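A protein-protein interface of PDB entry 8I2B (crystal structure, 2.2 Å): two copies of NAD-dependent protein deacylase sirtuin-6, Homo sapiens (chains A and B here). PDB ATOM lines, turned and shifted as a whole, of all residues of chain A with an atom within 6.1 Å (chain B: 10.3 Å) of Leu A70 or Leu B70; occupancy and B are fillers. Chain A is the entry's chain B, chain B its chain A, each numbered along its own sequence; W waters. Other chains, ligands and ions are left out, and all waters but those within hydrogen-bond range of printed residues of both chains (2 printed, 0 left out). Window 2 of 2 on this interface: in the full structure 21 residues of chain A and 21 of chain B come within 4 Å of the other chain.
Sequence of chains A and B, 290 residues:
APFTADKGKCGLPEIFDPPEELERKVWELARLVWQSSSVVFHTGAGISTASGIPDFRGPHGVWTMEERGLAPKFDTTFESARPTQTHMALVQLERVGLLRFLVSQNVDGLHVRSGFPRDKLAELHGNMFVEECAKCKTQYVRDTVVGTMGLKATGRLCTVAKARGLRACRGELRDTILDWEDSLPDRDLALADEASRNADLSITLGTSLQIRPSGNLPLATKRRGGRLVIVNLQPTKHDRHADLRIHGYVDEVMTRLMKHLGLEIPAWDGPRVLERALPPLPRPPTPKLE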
ATOM      1  N   HIS A  60      -7.656 -14.873  36.691  1.00  0.00           N
ATOM      2  CA  HIS A  60      -7.935 -16.272  36.273  1.00  0.00           C
ATOM      3  C   HIS A  60      -8.685 -17.012  37.393  1.00  0.00           C
ATOM      4  O   HIS A  60      -8.748 -18.249  37.387  1.00  0.00           O
ATOM      5  CB  HIS A  60      -6.648 -16.955  35.766  1.00  0.00           C
ATOM      6  CG  HIS A  60      -6.070 -16.280  34.559  1.00  0.00           C
ATOM      7  ND1 HIS A  60      -4.868 -16.655  34.009  1.00  0.00           N
ATOM      8  CD2 HIS A  60      -6.492 -15.225  33.817  1.00  0.00           C
ATOM      9  CE1 HIS A  60      -4.585 -15.877  32.980  1.00  0.00           C
ATOM     10  NE2 HIS A  60      -5.547 -14.970  32.856  1.00  0.00           N
ATOM     11  N   VAL A  62     -11.738 -18.768  39.621  1.00  0.00           N
ATOM     12  CA  VAL A  62     -12.869 -19.704  39.349  1.00  0.00           C
ATOM     13  C   VAL A  62     -14.058 -18.925  38.762  1.00  0.00           C
ATOM     14  O   VAL A  62     -14.511 -19.288  37.673  1.00  0.00           O
ATOM     15  CB  VAL A  62     -13.297 -20.453  40.620  1.00  0.00           C
ATOM     16  CG1 VAL A  62     -14.551 -21.272  40.367  1.00  0.00           C
ATOM     17  CG2 VAL A  62     -12.200 -21.346  41.173  1.00  0.00           C
ATOM     18  N   MET A  65     -13.345 -16.797  35.449  1.00  0.00           N
ATOM     19  CA  MET A  65     -13.224 -17.594  34.202  1.00  0.00           C
ATOM     20  C   MET A  65     -14.614 -18.093  33.804  1.00  0.00           C
ATOM     21  O   MET A  65     -14.930 -18.066  32.617  1.00  0.00           O
ATOM     22  CB  MET A  65     -12.235 -18.750  34.374  1.00  0.00           C
ATOM     23  CG  MET A  65     -10.810 -18.272  34.642  1.00  0.00           C
ATOM     24  SD  MET A  65     -10.121 -17.096  33.420  1.00  0.00           S
ATOM     25  CE  MET A  65      -9.211 -18.243  32.389  1.00  0.00           C
ATOM     26  N   GLU A  66     -15.438 -18.491  34.762  1.00  0.00           N
ATOM     27  CA  GLU A  66     -16.794 -19.023  34.457  1.00  0.00           C
ATOM     28  C   GLU A  66     -17.668 -17.897  33.869  1.00  0.00           C
ATOM     29  O   GLU A  66     -18.414 -18.189  32.925  1.00  0.00           O
ATOM     30  CB  GLU A  66     -17.314 -19.771  35.682  1.00  0.00           C
ATOM     31  CG  GLU A  66     -16.642 -21.134  35.807  1.00  0.00           C
ATOM     32  CD  GLU A  66     -17.008 -22.000  37.000  1.00  0.00           C
ATOM     33  OE1 GLU A  66     -18.160 -21.919  37.475  1.00  0.00           O
ATOM     34  OE2 GLU A  66     -16.127 -22.764  37.457  1.00  0.00           O
ATOM     35  N   GLU A  67     -17.531 -16.651  34.343  1.00  0.00           N
ATOM     36  CA  GLU A  67     -18.188 -15.432  33.787  1.00  0.00           C
ATOM     37  C   GLU A  67     -17.819 -15.265  32.306  1.00  0.00           C
ATOM     38  O   GLU A  67     -18.654 -14.762  31.555  1.00  0.00           O
ATOM     39  CB  GLU A  67     -17.731 -14.199  34.568  1.00  0.00           C
ATOM     40  CG  GLU A  67     -18.503 -12.926  34.299  1.00  0.00           C
ATOM     41  CD  GLU A  67     -17.776 -11.667  34.752  1.00  0.00           C
ATOM     42  OE1 GLU A  67     -16.621 -11.780  35.215  1.00  0.00           O
ATOM     43  OE2 GLU A  67     -18.363 -10.570  34.637  1.00  0.00           O
ATOM     44  N   ARG A  68     -16.601 -15.639  31.910  1.00  0.00           N
ATOM     45  CA  ARG A  68     -16.093 -15.520  30.514  1.00  0.00           C
ATOM     46  C   ARG A  68     -16.203 -16.857  29.762  1.00  0.00           C
ATOM     47  O   ARG A  68     -15.587 -16.967  28.688  1.00  0.00           O
ATOM     48  CB  ARG A  68     -14.628 -15.065  30.522  1.00  0.00           C
ATOM     49  CG  ARG A  68     -14.435 -13.577  30.781  1.00  0.00           C
ATOM     50  CD  ARG A  68     -13.009 -13.278  31.200  1.00  0.00           C
ATOM     51  NE  ARG A  68     -12.539 -11.970  30.755  1.00  0.00           N
ATOM     52  CZ  ARG A  68     -11.260 -11.602  30.702  1.00  0.00           C
ATOM     53  NH1 ARG A  68     -10.937 -10.387  30.283  1.00  0.00           N
ATOM     54  NH2 ARG A  68     -10.305 -12.445  31.063  1.00  0.00           N
ATOM     55  N   GLY A  69     -16.911 -17.856  30.297  1.00  0.00           N
ATOM     56  CA  GLY A  69     -17.053 -19.187  29.667  1.00  0.00           C
ATOM     57  C   GLY A  69     -15.761 -20.003  29.627  1.00  0.00           C
ATOM     58  O   GLY A  69     -15.674 -20.938  28.812  1.00  0.00           O
ATOM     59  N   LEU A  70     -14.783 -19.700  30.480  1.00  0.00           N
ATOM     60  CA  LEU A  70     -13.484 -20.423  30.531  1.00  0.00           C
ATOM     61  C   LEU A  70     -13.473 -21.248  31.811  1.00  0.00           C
ATOM     62  O   LEU A  70     -14.433 -21.104  32.599  1.00  0.00           O
ATOM     63  CB  LEU A  70     -12.327 -19.422  30.498  1.00  0.00           C
ATOM     64  CG  LEU A  70     -12.420 -18.387  29.379  1.00  0.00           C
ATOM     65  CD1 LEU A  70     -11.308 -17.351  29.473  1.00  0.00           C
ATOM     66  CD2 LEU A  70     -12.410 -19.075  28.019  1.00  0.00           C
ATOM     67  N   ALA A  71     -12.430 -22.059  32.000  1.00  0.00           N
ATOM     68  CA  ALA A  71     -12.267 -22.962  33.161  1.00  0.00           C
ATOM     69  C   ALA A  71     -11.239 -22.363  34.118  1.00  0.00           C
ATOM     70  O   ALA A  71     -10.371 -21.596  33.704  1.00  0.00           O
ATOM     71  CB  ALA A  71     -11.877 -24.340  32.698  1.00  0.00           C
ATOM     72  N   PRO A  72     -11.330 -22.649  35.438  1.00  0.00           N
ATOM     73  CA  PRO A  72     -10.202 -22.404  36.327  1.00  0.00           C
ATOM     74  C   PRO A  72      -9.154 -23.472  35.991  1.00  0.00           C
ATOM     75  O   PRO A  72      -9.514 -24.628  35.588  1.00  0.00           O
ATOM     76  CB  PRO A  72     -10.808 -22.585  37.722  1.00  0.00           C
ATOM     77  CG  PRO A  72     -11.891 -23.633  37.502  1.00  0.00           C
ATOM     78  CD  PRO A  72     -12.464 -23.284  36.142  1.00  0.00           C
ATOM     79  N   PHE B  56       4.303 -21.917  28.638  1.00  0.00           N
ATOM     80  CA  PHE B  56       4.175 -21.282  27.298  1.00  0.00           C
ATOM     81  C   PHE B  56       2.928 -21.787  26.547  1.00  0.00           C
ATOM     82  O   PHE B  56       2.193 -20.917  26.058  1.00  0.00           O
ATOM     83  CB  PHE B  56       5.485 -21.435  26.521  1.00  0.00           C
ATOM     84  CG  PHE B  56       6.578 -20.628  27.183  1.00  0.00           C
ATOM     85  CD1 PHE B  56       6.694 -19.269  26.940  1.00  0.00           C
ATOM     86  CD2 PHE B  56       7.434 -21.206  28.115  1.00  0.00           C
ATOM     87  CE1 PHE B  56       7.633 -18.493  27.608  1.00  0.00           C
ATOM     88  CE2 PHE B  56       8.401 -20.442  28.746  1.00  0.00           C
ATOM     89  CZ  PHE B  56       8.483 -19.089  28.524  1.00  0.00           C
ATOM     90  N   GLY B  58       0.631 -24.519  27.640  1.00  0.00           N
ATOM     91  CA  GLY B  58      -0.460 -25.097  28.459  1.00  0.00           C
ATOM     92  C   GLY B  58      -1.773 -24.322  28.290  1.00  0.00           C
ATOM     93  O   GLY B  58      -1.821 -23.242  27.713  1.00  0.00           O
ATOM     94  N   PRO B  59      -2.883 -24.792  28.886  1.00  0.00           N
ATOM     95  CA  PRO B  59      -4.176 -24.142  28.673  1.00  0.00           C
ATOM     96  C   PRO B  59      -4.147 -22.625  28.940  1.00  0.00           C
ATOM     97  O   PRO B  59      -4.718 -21.847  28.164  1.00  0.00           O
ATOM     98  CB  PRO B  59      -5.117 -24.884  29.625  1.00  0.00           C
ATOM     99  CG  PRO B  59      -4.443 -26.203  29.911  1.00  0.00           C
ATOM    100  CD  PRO B  59      -2.949 -26.011  29.714  1.00  0.00           C
ATOM    101  N   HIS B  60      -3.454 -22.213  29.985  1.00  0.00           N
ATOM    102  CA  HIS B  60      -3.195 -20.809  30.367  1.00  0.00           C
ATOM    103  C   HIS B  60      -1.740 -20.440  30.094  1.00  0.00           C
ATOM    104  O   HIS B  60      -1.288 -19.377  30.556  1.00  0.00           O
ATOM    105  CB  HIS B  60      -3.668 -20.534  31.797  1.00  0.00           C
ATOM    106  CG  HIS B  60      -5.122 -20.793  32.014  1.00  0.00           C
ATOM    107  ND1 HIS B  60      -5.703 -20.660  33.265  1.00  0.00           N
ATOM    108  CD2 HIS B  60      -6.110 -21.193  31.170  1.00  0.00           C
ATOM    109  CE1 HIS B  60      -6.994 -20.957  33.176  1.00  0.00           C
ATOM    110  NE2 HIS B  60      -7.260 -21.327  31.909  1.00  0.00           N
ATOM    111  N   GLY B  61      -1.081 -21.138  29.188  1.00  0.00           N
ATOM    112  CA  GLY B  61       0.287 -20.733  28.798  1.00  0.00           C
ATOM    113  C   GLY B  61       0.404 -19.328  28.181  1.00  0.00           C
ATOM    114  O   GLY B  61      -0.571 -18.821  27.594  1.00  0.00           O
ATOM    115  N   VAL B  62       1.592 -18.724  28.271  1.00  0.00           N
ATOM    116  CA  VAL B  62       1.923 -17.396  27.678  1.00  0.00           C
ATOM    117  C   VAL B  62       1.445 -17.352  26.208  1.00  0.00           C
ATOM    118  O   VAL B  62       0.682 -16.441  25.852  1.00  0.00           O
ATOM    119  CB  VAL B  62       3.431 -17.114  27.742  1.00  0.00           C
ATOM    120  CG1 VAL B  62       3.767 -15.843  26.956  1.00  0.00           C
ATOM    121  CG2 VAL B  62       3.939 -17.023  29.183  1.00  0.00           C
ATOM    122  N   TRP B  63       1.922 -18.269  25.363  1.00  0.00           N
ATOM    123  CA  TRP B  63       1.586 -18.260  23.913  1.00  0.00           C
ATOM    124  C   TRP B  63       0.100 -18.600  23.742  1.00  0.00           C
ATOM    125  O   TRP B  63      -0.580 -17.954  22.925  1.00  0.00           O
ATOM    126  CB  TRP B  63       2.447 -19.242  23.116  1.00  0.00           C
ATOM    127  CG  TRP B  63       3.935 -19.080  23.184  1.00  0.00           C
ATOM    128  CD1 TRP B  63       4.820 -20.087  22.936  1.00  0.00           C
ATOM    129  CD2 TRP B  63       4.736 -17.896  23.360  1.00  0.00           C
ATOM    130  NE1 TRP B  63       6.099 -19.635  22.968  1.00  0.00           N
ATOM    131  CE2 TRP B  63       6.094 -18.297  23.244  1.00  0.00           C
ATOM    132  CE3 TRP B  63       4.459 -16.547  23.616  1.00  0.00           C
ATOM    133  CZ2 TRP B  63       7.160 -17.421  23.431  1.00  0.00           C
ATOM    134  CZ3 TRP B  63       5.513 -15.679  23.802  1.00  0.00           C
ATOM    135  CH2 TRP B  63       6.841 -16.105  23.698  1.00  0.00           C
ATOM    136  N   THR B  64      -0.388 -19.620  24.447  1.00  0.00           N
ATOM    137  CA  THR B  64      -1.821 -20.032  24.379  1.00  0.00           C
ATOM    138  C   THR B  64      -2.703 -18.794  24.603  1.00  0.00           C
ATOM    139  O   THR B  64      -3.602 -18.590  23.807  1.00  0.00           O
ATOM    140  CB  THR B  64      -2.146 -21.145  25.368  1.00  0.00           C
ATOM    141  OG1 THR B  64      -1.169 -22.161  25.153  1.00  0.00           O
ATOM    142  CG2 THR B  64      -3.569 -21.644  25.252  1.00  0.00           C
ATOM    143  N   MET B  65      -2.443 -17.990  25.626  1.00  0.00           N
ATOM    144  CA  MET B  65      -3.362 -16.897  26.020  1.00  0.00           C
ATOM    145  C   MET B  65      -3.246 -15.760  24.996  1.00  0.00           C
ATOM    146  O   MET B  65      -4.280 -15.172  24.598  1.00  0.00           O
ATOM    147  CB  MET B  65      -3.034 -16.394  27.421  1.00  0.00           C
ATOM    148  CG  MET B  65      -3.261 -17.424  28.521  1.00  0.00           C
ATOM    149  SD  MET B  65      -4.962 -18.060  28.556  1.00  0.00           S
ATOM    150  CE  MET B  65      -5.702 -16.961  29.756  1.00  0.00           C
ATOM    151  N   GLU B  66      -2.034 -15.497  24.524  1.00  0.00           N
ATOM    152  CA  GLU B  66      -1.777 -14.488  23.483  1.00  0.00           C
ATOM    153  C   GLU B  66      -2.641 -14.783  22.235  1.00  0.00           C
ATOM    154  O   GLU B  66      -3.201 -13.836  21.667  1.00  0.00           O
ATOM    155  CB  GLU B  66      -0.270 -14.521  23.234  1.00  0.00           C
ATOM    156  CG  GLU B  66       0.206 -13.703  22.061  1.00  0.00           C
ATOM    157  CD  GLU B  66       1.707 -13.484  22.104  1.00  0.00           C
ATOM    158  OE1 GLU B  66       2.396 -13.831  21.117  1.00  0.00           O
ATOM    159  OE2 GLU B  66       2.188 -13.007  23.156  1.00  0.00           O
ATOM    160  N   GLU B  67      -2.747 -16.049  21.849  1.00  0.00           N
ATOM    161  CA  GLU B  67      -3.516 -16.552  20.688  1.00  0.00           C
ATOM    162  C   GLU B  67      -4.989 -16.179  20.861  1.00  0.00           C
ATOM    163  O   GLU B  67      -5.643 -15.961  19.852  1.00  0.00           O
ATOM    164  CB  GLU B  67      -3.464 -18.083  20.621  1.00  0.00           C
ATOM    165  CG  GLU B  67      -2.501 -18.669  19.621  1.00  0.00           C
ATOM    166  CD  GLU B  67      -2.574 -20.191  19.598  1.00  0.00           C
ATOM    167  OE1 GLU B  67      -3.623 -20.734  20.021  1.00  0.00           O
ATOM    168  OE2 GLU B  67      -1.578 -20.840  19.185  1.00  0.00           O
ATOM    169  N   ARG B  68      -5.496 -16.181  22.105  1.00  0.00           N
ATOM    170  CA  ARG B  68      -6.920 -15.877  22.415  1.00  0.00           C
ATOM    171  C   ARG B  68      -7.098 -14.406  22.824  1.00  0.00           C
ATOM    172  O   ARG B  68      -8.184 -14.078  23.363  1.00  0.00           O
ATOM    173  CB  ARG B  68      -7.415 -16.783  23.553  1.00  0.00           C
ATOM    174  CG  ARG B  68      -7.789 -18.198  23.143  1.00  0.00           C
ATOM    175  CD  ARG B  68      -6.597 -19.115  23.023  1.00  0.00           C
ATOM    176  NE  ARG B  68      -6.928 -20.544  23.027  1.00  0.00           N
ATOM    177  CZ  ARG B  68      -6.157 -21.517  22.519  1.00  0.00           C
ATOM    178  NH1 ARG B  68      -5.002 -21.218  21.940  1.00  0.00           N
ATOM    179  NH2 ARG B  68      -6.546 -22.786  22.575  1.00  0.00           N
ATOM    180  N   GLY B  69      -6.089 -13.550  22.655  1.00  0.00           N
ATOM    181  CA  GLY B  69      -6.196 -12.129  23.052  1.00  0.00           C
ATOM    182  C   GLY B  69      -6.160 -11.921  24.578  1.00  0.00           C
ATOM    183  O   GLY B  69      -6.563 -10.834  25.037  1.00  0.00           O
ATOM    184  N   LEU B  70      -5.700 -12.898  25.359  1.00  0.00           N
ATOM    185  CA  LEU B  70      -5.705 -12.826  26.849  1.00  0.00           C
ATOM    186  C   LEU B  70      -4.263 -12.740  27.312  1.00  0.00           C
ATOM    187  O   LEU B  70      -3.385 -12.859  26.446  1.00  0.00           O
ATOM    188  CB  LEU B  70      -6.388 -14.059  27.443  1.00  0.00           C
ATOM    189  CG  LEU B  70      -7.764 -14.361  26.870  1.00  0.00           C
ATOM    190  CD1 LEU B  70      -8.335 -15.661  27.438  1.00  0.00           C
ATOM    191  CD2 LEU B  70      -8.711 -13.209  27.090  1.00  0.00           C
ATOM    192  N   ALA B  71      -4.062 -12.492  28.604  1.00  0.00           N
ATOM    193  CA  ALA B  71      -2.736 -12.374  29.254  1.00  0.00           C
ATOM    194  C   ALA B  71      -2.503 -13.624  30.091  1.00  0.00           C
ATOM    195  O   ALA B  71      -3.452 -14.212  30.618  1.00  0.00           O
ATOM    196  CB  ALA B  71      -2.663 -11.115  30.096  1.00  0.00           C
ATOM    197  N   PRO B  72      -1.234 -14.071  30.247  1.00  0.00           N
ATOM    198  CA  PRO B  72      -0.918 -15.108  31.214  1.00  0.00           C
ATOM    199  C   PRO B  72      -0.948 -14.459  32.597  1.00  0.00           C
ATOM    200  O   PRO B  72      -0.845 -13.256  32.676  1.00  0.00           O
ATOM    201  CB  PRO B  72       0.483 -15.558  30.791  1.00  0.00           C
ATOM    202  CG  PRO B  72       1.099 -14.273  30.301  1.00  0.00           C
ATOM    203  CD  PRO B  72      -0.036 -13.641  29.503  1.00  0.00           C
ATOM    204  N   LYS B  73      -1.068 -15.270  33.637  1.00  0.00           N
ATOM    205  CA  LYS B  73      -1.093 -14.775  35.039  1.00  0.00           C
ATOM    206  C   LYS B  73       0.116 -15.361  35.786  1.00  0.00           C
ATOM    207  O   LYS B  73       0.410 -16.568  35.615  1.00  0.00           O
ATOM    208  CB  LYS B  73      -2.450 -15.102  35.663  1.00  0.00           C
ATOM    209  CG  LYS B  73      -2.467 -15.055  37.175  1.00  0.00           C
ATOM    210  CD  LYS B  73      -3.295 -13.959  37.739  1.00  0.00           C
ATOM    211  CE  LYS B  73      -3.252 -13.929  39.255  1.00  0.00           C
ATOM    212  NZ  LYS B  73      -2.350 -12.876  39.769  1.00  0.00           N
HETATM  213  O   HOH W   1      -1.847 -17.631  32.971  1.00  0.00           O
HETATM  214  O   HOH W   2      -6.357 -12.689  31.137  1.00  0.00           O
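Leu A70 touches one residue of chain B. Leu B70 touches just one residue of chain A: Leu A70 (3.98 Å). No residue of chain B comes within 4 Å of Glu A66. No residue of chain B comes within 4 Å of Arg A68. No residue of chain B comes within 4 Å of Gly A69. Of the printed residues of chain B, Ala A71 touches His B60 (3.5 Å). Of the printed residues of chain A, Met B65 touches His A60 (3.6 Å). Printed residues of chain A within 4 Å of His B60: Met A65 (3.6 Å) and Ala A71 (3.5 Å). Glu B66 touches none of the printed residues of chain A. The nearest residue of chain B that does not touch Leu A70 is His B60 (5.6 Å). The nearest residue of chain A that does not touch Leu B70 is Arg A68 (4.3 Å).
A ring nitrogen (NE2) of His A60 sits close to the backbone carbonyl oxygen of Ala B71, at 3.2 Å.
His A60 touches Met B65, and with the chains exchanged Met A65 touches His B60. His A60 touches Ala B71, and with the chains exchanged Ala A71 touches His B60. His A60 touches Pro B72, but with the chains exchanged Pro A72 does not touch His B60 (4.3 Å). Leu B70 touches its own counterpart, Leu A70. 10 positions are printed for both chains. Of the 7 pairs that touch across the chains among the printed residues, 5 have their exchanged pair printed and touching as well.
Water W1 lies within hydrogen-bond range of N of Lys B73 (2.6 Å), O of His B60 (3.0 Å) and ND1 of His A60 (3.3 Å). Water W2 lies within hydrogen-bond range of a ring nitrogen (NE2) of His A60 (3.0 Å) and the backbone carbonyl oxygen (O) of Ala B71 (3.3 Å).
His A60 touches Met B65. CE1 of His A60 touches C of Pro B72, 3.9 Å away. ND1 of His A60 touches CB of Lys B73, 3.3 Å away. Met A65 touches His B60 (CE to CE1, 3.6 Å). Leu B70 touches Leu A70. His B60 touches Ala A71.
Of the 17 printed residues of chain B, 6 touch a printed residue of chain A. Hydrophobic or aromatic side chains of chain B that line the printed part of chain A: His B60, Met B65 and Leu B70. Of the 10 printed residues of chain A, 4 touch a printed residue of chain B. Along chain A the printed residues that touch a printed residue of chain B span positions 60 to 71. Among the printed residues, 7 pairs touch across the chains. Among the printed residues, no Asp or Glu carboxylate lies within 4 Å of a Lys or Arg side-chain nitrogen of the other chain.
The backbone NH (N) of Leu A70 lies within hydrogen-bond range of the backbone carbonyl oxygen (O) of Met A65 (2.7 Å). The backbone carbonyl oxygen (O) of Met B65 lies within hydrogen-bond range of the backbone NH (N) of Leu B70, 2.8 Å away.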
